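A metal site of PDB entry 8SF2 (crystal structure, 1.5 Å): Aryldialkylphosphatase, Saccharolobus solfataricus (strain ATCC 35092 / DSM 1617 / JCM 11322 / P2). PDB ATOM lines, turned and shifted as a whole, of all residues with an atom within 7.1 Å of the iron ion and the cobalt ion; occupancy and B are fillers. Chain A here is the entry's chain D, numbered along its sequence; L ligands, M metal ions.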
ATOM      1  N   HIS A  22      21.260   6.039 -17.803  1.00  0.00           N
ATOM      2  CA  HIS A  22      21.433   5.966 -16.355  1.00  0.00           C
ATOM      3  C   HIS A  22      20.769   4.698 -15.809  1.00  0.00           C
ATOM      4  O   HIS A  22      19.597   4.714 -15.422  1.00  0.00           O
ATOM      5  CB  HIS A  22      20.905   7.223 -15.670  1.00  0.00           C
ATOM      6  CG  HIS A  22      21.285   7.345 -14.221  1.00  0.00           C
ATOM      7  ND1 HIS A  22      21.698   8.540 -13.676  1.00  0.00           N
ATOM      8  CD2 HIS A  22      21.282   6.455 -13.213  1.00  0.00           C
ATOM      9  CE1 HIS A  22      21.955   8.365 -12.387  1.00  0.00           C
ATOM     10  NE2 HIS A  22      21.712   7.107 -12.077  1.00  0.00           N
ATOM     11  N   GLU A  23      21.537   3.603 -15.767  1.00  0.00           N
ATOM     12  CA  GLU A  23      21.107   2.348 -15.188  1.00  0.00           C
ATOM     13  C   GLU A  23      22.273   1.755 -14.391  1.00  0.00           C
ATOM     14  O   GLU A  23      23.434   2.063 -14.661  1.00  0.00           O
ATOM     15  CB  GLU A  23      20.699   1.330 -16.264  1.00  0.00           C
ATOM     16  CG  GLU A  23      19.736   1.892 -17.304  1.00  0.00           C
ATOM     17  CD  GLU A  23      18.344   2.214 -16.790  1.00  0.00           C
ATOM     18  OE1 GLU A  23      17.647   3.003 -17.449  1.00  0.00           O
ATOM     19  OE2 GLU A  23      17.963   1.683 -15.729  1.00  0.00           O
ATOM     20  N   HIS A  24      21.955   0.912 -13.420  1.00  0.00           N
ATOM     21  CA  HIS A  24      22.968   0.303 -12.566  1.00  0.00           C
ATOM     22  C   HIS A  24      22.870  -1.212 -12.640  1.00  0.00           C
ATOM     23  O   HIS A  24      21.844  -1.796 -12.285  1.00  0.00           O
ATOM     24  CB  HIS A  24      22.777   0.725 -11.109  1.00  0.00           C
ATOM     25  CG  HIS A  24      22.914   2.192 -10.865  1.00  0.00           C
ATOM     26  ND1 HIS A  24      24.111   2.819 -10.619  1.00  0.00           N
ATOM     27  CD2 HIS A  24      21.964   3.155 -10.785  1.00  0.00           C
ATOM     28  CE1 HIS A  24      23.896   4.112 -10.417  1.00  0.00           C
ATOM     29  NE2 HIS A  24      22.600   4.342 -10.512  1.00  0.00           N
ATOM     30  N   PRO A  67      26.363   4.683 -14.177  1.00  0.00           N
ATOM     31  CA  PRO A  67      27.092   5.638 -13.334  1.00  0.00           C
ATOM     32  C   PRO A  67      27.332   5.173 -11.902  1.00  0.00           C
ATOM     33  O   PRO A  67      27.316   5.972 -10.973  1.00  0.00           O
ATOM     34  CB  PRO A  67      26.188   6.871 -13.375  1.00  0.00           C
ATOM     35  CG  PRO A  67      24.790   6.301 -13.485  1.00  0.00           C
ATOM     36  CD  PRO A  67      24.927   4.995 -14.259  1.00  0.00           C
ATOM     37  N   THR A  68      27.564   3.870 -11.731  1.00  0.00           N
ATOM     38  CA  THR A  68      27.999   3.337 -10.444  1.00  0.00           C
ATOM     39  C   THR A  68      29.469   3.696 -10.245  1.00  0.00           C
ATOM     40  O   THR A  68      30.319   3.301 -11.055  1.00  0.00           O
ATOM     41  CB  THR A  68      27.833   1.808 -10.403  1.00  0.00           C
ATOM     42  OG1 THR A  68      26.517   1.436 -10.804  1.00  0.00           O
ATOM     43  CG2 THR A  68      28.105   1.258  -9.015  1.00  0.00           C
ATOM     44  N   LEU A  72      28.899   3.695  -4.436  1.00  0.00           N
ATOM     45  CA  LEU A  72      27.829   2.837  -4.933  1.00  0.00           C
ATOM     46  C   LEU A  72      28.335   1.456  -5.320  1.00  0.00           C
ATOM     47  O   LEU A  72      27.542   0.647  -5.820  1.00  0.00           O
ATOM     48  CB  LEU A  72      27.162   3.501  -6.146  1.00  0.00           C
ATOM     49  CG  LEU A  72      26.558   4.889  -5.927  1.00  0.00           C
ATOM     50  CD1 LEU A  72      26.128   5.510  -7.243  1.00  0.00           C
ATOM     51  CD2 LEU A  72      25.374   4.815  -4.969  1.00  0.00           C
ATOM     52  N   TYR A  97      30.420   9.519  -5.317  1.00  0.00           N
ATOM     53  CA  TYR A  97      29.039   9.722  -4.925  1.00  0.00           C
ATOM     54  C   TYR A  97      29.008   9.916  -3.407  1.00  0.00           C
ATOM     55  O   TYR A  97      29.143   8.958  -2.653  1.00  0.00           O
ATOM     56  CB  TYR A  97      28.223   8.505  -5.372  1.00  0.00           C
ATOM     57  CG  TYR A  97      26.742   8.568  -5.144  1.00  0.00           C
ATOM     58  CD1 TYR A  97      26.187   8.248  -3.912  1.00  0.00           C
ATOM     59  CD2 TYR A  97      25.880   8.855  -6.186  1.00  0.00           C
ATOM     60  CE1 TYR A  97      24.824   8.259  -3.711  1.00  0.00           C
ATOM     61  CE2 TYR A  97      24.506   8.860  -6.006  1.00  0.00           C
ATOM     62  CZ  TYR A  97      23.977   8.559  -4.765  1.00  0.00           C
ATOM     63  OH  TYR A  97      22.616   8.557  -4.584  1.00  0.00           O
ATOM     64  N   TYR A  99      27.015  12.712  -0.299  1.00  0.00           N
ATOM     65  CA  TYR A  99      26.042  13.759  -0.012  1.00  0.00           C
ATOM     66  C   TYR A  99      26.611  14.803   0.942  1.00  0.00           C
ATOM     67  O   TYR A  99      26.160  15.947   0.911  1.00  0.00           O
ATOM     68  CB  TYR A  99      24.768  13.183   0.616  1.00  0.00           C
ATOM     69  CG  TYR A  99      23.900  12.337  -0.296  1.00  0.00           C
ATOM     70  CD1 TYR A  99      24.230  12.100  -1.619  1.00  0.00           C
ATOM     71  CD2 TYR A  99      22.729  11.777   0.195  1.00  0.00           C
ATOM     72  CE1 TYR A  99      23.424  11.311  -2.434  1.00  0.00           C
ATOM     73  CE2 TYR A  99      21.916  10.992  -0.608  1.00  0.00           C
ATOM     74  CZ  TYR A  99      22.268  10.750  -1.926  1.00  0.00           C
ATOM     75  OH  TYR A  99      21.445   9.963  -2.710  1.00  0.00           O
ATOM     76  N   KCX A 137      30.855  10.961 -12.739  1.00  0.00           N
ATOM     77  CA  KCX A 137      29.605  11.007 -11.952  1.00  0.00           C
ATOM     78  CB  KCX A 137      29.102   9.588 -11.691  1.00  0.00           C
ATOM     79  CG  KCX A 137      27.957   9.500 -10.690  1.00  0.00           C
ATOM     80  CD  KCX A 137      26.695  10.153 -11.197  1.00  0.00           C
ATOM     81  CE  KCX A 137      25.531   9.992 -10.237  1.00  0.00           C
ATOM     82  NZ  KCX A 137      25.108   8.589 -10.136  1.00  0.00           N
ATOM     83  C   KCX A 137      29.863  11.746 -10.637  1.00  0.00           C
ATOM     84  O   KCX A 137      30.800  11.384  -9.927  1.00  0.00           O
ATOM     85  CX  KCX A 137      23.887   8.274  -9.706  1.00  0.00           C
ATOM     86  OQ1 KCX A 137      23.638   6.992  -9.662  1.00  0.00           O
ATOM     87  OQ2 KCX A 137      23.060   9.112  -9.362  1.00  0.00           O
ATOM     88  N   ILE A 138      28.989  12.757 -10.349  1.00  0.00           N
ATOM     89  CA  ILE A 138      29.056  13.520  -9.077  1.00  0.00           C
ATOM     90  C   ILE A 138      27.641  13.562  -8.502  1.00  0.00           C
ATOM     91  O   ILE A 138      26.669  13.310  -9.221  1.00  0.00           O
ATOM     92  CB  ILE A 138      29.615  14.930  -9.310  1.00  0.00           C
ATOM     93  CG1 ILE A 138      28.687  15.736 -10.218  1.00  0.00           C
ATOM     94  CG2 ILE A 138      31.016  14.876  -9.873  1.00  0.00           C
ATOM     95  CD1 ILE A 138      29.100  17.173 -10.426  1.00  0.00           C
ATOM     96  N   ALA A 139      27.525  13.894  -7.213  1.00  0.00           N
ATOM     97  CA  ALA A 139      26.235  13.897  -6.530  1.00  0.00           C
ATOM     98  C   ALA A 139      26.119  15.073  -5.559  1.00  0.00           C
ATOM     99  O   ALA A 139      27.107  15.578  -5.032  1.00  0.00           O
ATOM    100  CB  ALA A 139      26.012  12.599  -5.778  1.00  0.00           C
ATOM    101  N   ASP A 141      22.577  16.133  -2.691  1.00  0.00           N
ATOM    102  CA  ASP A 141      21.211  15.802  -2.351  1.00  0.00           C
ATOM    103  C   ASP A 141      20.700  16.778  -1.304  1.00  0.00           C
ATOM    104  O   ASP A 141      20.989  17.977  -1.387  1.00  0.00           O
ATOM    105  CB  ASP A 141      21.100  14.328  -1.931  1.00  0.00           C
ATOM    106  CG  ASP A 141      19.718  13.746  -2.154  1.00  0.00           C
ATOM    107  OD1 ASP A 141      18.804  14.012  -1.339  1.00  0.00           O
ATOM    108  OD2 ASP A 141      19.540  13.025  -3.166  1.00  0.00           O
ATOM    109  N   THR A 169      25.273  13.954 -13.316  1.00  0.00           N
ATOM    110  CA  THR A 169      25.069  14.262 -11.913  1.00  0.00           C
ATOM    111  C   THR A 169      23.883  13.508 -11.328  1.00  0.00           C
ATOM    112  O   THR A 169      22.960  13.084 -12.040  1.00  0.00           O
ATOM    113  CB  THR A 169      24.890  15.767 -11.636  1.00  0.00           C
ATOM    114  OG1 THR A 169      23.504  16.113 -11.764  1.00  0.00           O
ATOM    115  CG2 THR A 169      25.738  16.637 -12.532  1.00  0.00           C
ATOM    116  N   HIS A 170      23.954  13.341 -10.016  1.00  0.00           N
ATOM    117  CA  HIS A 170      22.820  13.038  -9.161  1.00  0.00           C
ATOM    118  C   HIS A 170      22.454  14.337  -8.452  1.00  0.00           C
ATOM    119  O   HIS A 170      23.340  14.989  -7.906  1.00  0.00           O
ATOM    120  CB  HIS A 170      23.230  11.996  -8.124  1.00  0.00           C
ATOM    121  CG  HIS A 170      22.245  11.781  -7.020  1.00  0.00           C
ATOM    122  ND1 HIS A 170      21.504  10.626  -6.952  1.00  0.00           N
ATOM    123  CD2 HIS A 170      21.879  12.525  -5.970  1.00  0.00           C
ATOM    124  CE1 HIS A 170      20.728  10.670  -5.879  1.00  0.00           C
ATOM    125  NE2 HIS A 170      20.932  11.818  -5.267  1.00  0.00           N
ATOM    126  N   SER A 171      21.167  14.702  -8.469  1.00  0.00           N
ATOM    127  CA  SER A 171      20.711  15.870  -7.727  1.00  0.00           C
ATOM    128  C   SER A 171      19.400  15.529  -7.023  1.00  0.00           C
ATOM    129  O   SER A 171      18.789  14.491  -7.280  1.00  0.00           O
ATOM    130  CB  SER A 171      20.557  17.093  -8.629  1.00  0.00           C
ATOM    131  OG  SER A 171      19.295  17.124  -9.274  1.00  0.00           O
ATOM    132  N   GLY A 198      20.943  15.276 -13.146  1.00  0.00           N
ATOM    133  CA  GLY A 198      20.185  14.073 -12.890  1.00  0.00           C
ATOM    134  C   GLY A 198      18.968  14.293 -12.004  1.00  0.00           C
ATOM    135  O   GLY A 198      18.927  15.223 -11.175  1.00  0.00           O
ATOM    136  N   HIS A 199      17.969  13.432 -12.215  1.00  0.00           N
ATOM    137  CA  HIS A 199      16.850  13.211 -11.315  1.00  0.00           C
ATOM    138  C   HIS A 199      15.845  14.352 -11.365  1.00  0.00           C
ATOM    139  O   HIS A 199      15.012  14.486 -10.467  1.00  0.00           O
ATOM    140  CB  HIS A 199      17.333  12.884  -9.904  1.00  0.00           C
ATOM    141  CG  HIS A 199      18.284  11.731  -9.856  1.00  0.00           C
ATOM    142  ND1 HIS A 199      18.290  10.732 -10.805  1.00  0.00           N
ATOM    143  CD2 HIS A 199      19.243  11.413  -8.985  1.00  0.00           C
ATOM    144  CE1 HIS A 199      19.246   9.854 -10.517  1.00  0.00           C
ATOM    145  NE2 HIS A 199      19.834  10.248  -9.414  1.00  0.00           N
ATOM    146  N   ASP A 222      14.962  10.452 -15.395  1.00  0.00           N
ATOM    147  CA  ASP A 222      15.850   9.293 -15.400  1.00  0.00           C
ATOM    148  C   ASP A 222      15.526   8.289 -14.298  1.00  0.00           C
ATOM    149  O   ASP A 222      16.329   7.385 -14.058  1.00  0.00           O
ATOM    150  CB  ASP A 222      17.311   9.749 -15.316  1.00  0.00           C
ATOM    151  CG  ASP A 222      17.631  10.633 -14.121  1.00  0.00           C
ATOM    152  OD1 ASP A 222      16.850  10.624 -13.146  1.00  0.00           O
ATOM    153  OD2 ASP A 222      18.665  11.329 -14.165  1.00  0.00           O
ATOM    154  N   ARG A 223      14.343   8.389 -13.687  1.00  0.00           N
ATOM    155  CA  ARG A 223      13.978   7.477 -12.616  1.00  0.00           C
ATOM    156  C   ARG A 223      12.593   6.871 -12.843  1.00  0.00           C
ATOM    157  O   ARG A 223      11.855   6.629 -11.891  1.00  0.00           O
ATOM    158  CB  ARG A 223      14.046   8.173 -11.249  1.00  0.00           C
ATOM    159  CG  ARG A 223      15.454   8.252 -10.692  1.00  0.00           C
ATOM    160  CD  ARG A 223      15.530   9.082  -9.423  1.00  0.00           C
ATOM    161  NE  ARG A 223      16.666   8.652  -8.621  1.00  0.00           N
ATOM    162  CZ  ARG A 223      17.004   9.187  -7.457  1.00  0.00           C
ATOM    163  NH1 ARG A 223      16.342  10.231  -6.970  1.00  0.00           N
ATOM    164  NH2 ARG A 223      18.020   8.677  -6.787  1.00  0.00           N
ATOM    165  N   ASP A 256      17.129   4.469 -13.891  1.00  0.00           N
ATOM    166  CA  ASP A 256      17.951   4.436 -12.688  1.00  0.00           C
ATOM    167  C   ASP A 256      17.715   3.108 -11.985  1.00  0.00           C
ATOM    168  O   ASP A 256      17.806   3.004 -10.762  1.00  0.00           O
ATOM    169  CB  ASP A 256      17.625   5.600 -11.752  1.00  0.00           C
ATOM    170  CG  ASP A 256      18.678   5.862 -10.685  1.00  0.00           C
ATOM    171  OD1 ASP A 256      19.798   5.305 -10.791  1.00  0.00           O
ATOM    172  OD2 ASP A 256      18.387   6.649  -9.754  1.00  0.00           O
ATOM    173  N   TYR A 257      17.381   2.092 -12.784  1.00  0.00           N
ATOM    174  CA  TYR A 257      17.054   0.805 -12.212  1.00  0.00           C
ATOM    175  C   TYR A 257      18.332   0.170 -11.700  1.00  0.00           C
ATOM    176  O   TYR A 257      19.344   0.130 -12.409  1.00  0.00           O
ATOM    177  CB  TYR A 257      16.386  -0.138 -13.199  1.00  0.00           C
ATOM    178  CG  TYR A 257      15.989  -1.450 -12.569  1.00  0.00           C
ATOM    179  CD1 TYR A 257      14.974  -1.504 -11.635  1.00  0.00           C
ATOM    180  CD2 TYR A 257      16.648  -2.625 -12.880  1.00  0.00           C
ATOM    181  CE1 TYR A 257      14.606  -2.694 -11.029  1.00  0.00           C
ATOM    182  CE2 TYR A 257      16.291  -3.827 -12.289  1.00  0.00           C
ATOM    183  CZ  TYR A 257      15.265  -3.856 -11.368  1.00  0.00           C
ATOM    184  OH  TYR A 257      14.903  -5.055 -10.790  1.00  0.00           O
ATOM    185  N   CYS A 258      18.278  -0.320 -10.466  1.00  0.00           N
ATOM    186  CA  CYS A 258      19.369  -1.071  -9.874  1.00  0.00           C
ATOM    187  C   CYS A 258      18.982  -2.536  -9.836  1.00  0.00           C
ATOM    188  O   CYS A 258      18.094  -2.926  -9.082  1.00  0.00           O
ATOM    189  CB  CYS A 258      19.679  -0.566  -8.466  1.00  0.00           C
ATOM    190  SG  CYS A 258      20.078   1.187  -8.414  1.00  0.00           S
ATOM    191  N   TRP A 263      20.461  -1.034  -0.307  1.00  0.00           N
ATOM    192  CA  TRP A 263      19.817  -0.073   0.582  1.00  0.00           C
ATOM    193  C   TRP A 263      18.563  -0.691   1.191  1.00  0.00           C
ATOM    194  O   TRP A 263      17.891  -1.511   0.554  1.00  0.00           O
ATOM    195  CB  TRP A 263      19.472   1.228  -0.167  1.00  0.00           C
ATOM    196  CG  TRP A 263      20.639   1.978  -0.736  1.00  0.00           C
ATOM    197  CD1 TRP A 263      21.944   1.561  -0.795  1.00  0.00           C
ATOM    198  CD2 TRP A 263      20.616   3.291  -1.334  1.00  0.00           C
ATOM    199  NE1 TRP A 263      22.729   2.526  -1.392  1.00  0.00           N
ATOM    200  CE2 TRP A 263      21.940   3.593  -1.734  1.00  0.00           C
ATOM    201  CE3 TRP A 263      19.606   4.226  -1.567  1.00  0.00           C
ATOM    202  CZ2 TRP A 263      22.269   4.802  -2.342  1.00  0.00           C
ATOM    203  CZ3 TRP A 263      19.931   5.425  -2.184  1.00  0.00           C
ATOM    204  CH2 TRP A 263      21.250   5.703  -2.564  1.00  0.00           C
HETATM  205  P1  LIG L   1      20.888   6.866  -7.797  1.00  0.00           P
HETATM  206  O1  LIG L   1      19.524   6.413  -7.272  1.00  0.00           O
HETATM  207  O2  LIG L   1      20.761   7.537  -9.142  1.00  0.00           O
HETATM  208  O3  LIG L   1      21.820   5.660  -7.865  1.00  0.00           O
HETATM  209  O4  LIG L   1      21.464   7.888  -6.868  1.00  0.00           O
HETATM  210 FE    FE M   1      21.738   6.190 -10.205  1.00  0.00          FE
HETATM  211 CO    CO M   2      21.296   9.163  -8.364  1.00  0.00          CO
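N of Asp 256 sits at hydrogen-bond distance from O of Asp 222 (3.0 Å). The backbone NH (N) of His 170 is in hydrogen-bond range of the backbone carbonyl oxygen (O) of Ile 138. A ring nitrogen (ND1) of His 170 sits close to the side-chain hydroxyl (OH) of Tyr 97, at 3.3 Å. A ring nitrogen (ND1) of His 199 is in hydrogen-bond range of the side-chain carboxylate (OD1) of Asp 222. NE2 of His 170 lies within hydrogen-bond range of OH of Tyr 99 (3.2 Å). The side-chain carboxylate (OD2) of Asp 256 is in salt-bridge range of the guanidinium group (NE) of Arg 223 (2.9 Å). The side-chain hydroxyl (OH) of Tyr 99 sits at hydrogen-bond distance from the side-chain hydroxyl (OH) of Tyr 97, 2.6 Å away. OG1 of Thr 68 sits at hydrogen-bond distance from ND1 of His 24, at 2.8 Å.
The cobalt ion is bound by O2 of the ligand (1.9 Å), O4 of the ligand (2.0 Å), OQ2 of KCX 137 (2.0 Å), ND1 of His 170 (2.0 Å) and NE2 of His 199 (2.1 Å). The cobalt ion has five donor atoms within binding distance.
Tyr 97 touches the cobalt ion (CE2 to CO, 3.99 Å). Arg 223 touches the cobalt ion. Within 4 Å of the cobalt ion: Tyr 97, KCX 137, His 170, His 199 and Arg 223.
The iron ion is bound by an oxygen (O2) of the ligand, a ring nitrogen (NE2) of His 24, a ring nitrogen (NE2) of His 22, OQ1 of KCX 137, the side-chain carboxylate (OD1) of Asp 256 and an oxygen (O3) of the ligand.
Of the 23 residues printed, 4 come within 4 Å of the iron ion. The nearest printed residue that does not touch the iron ion is His 199 (4.4 Å).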
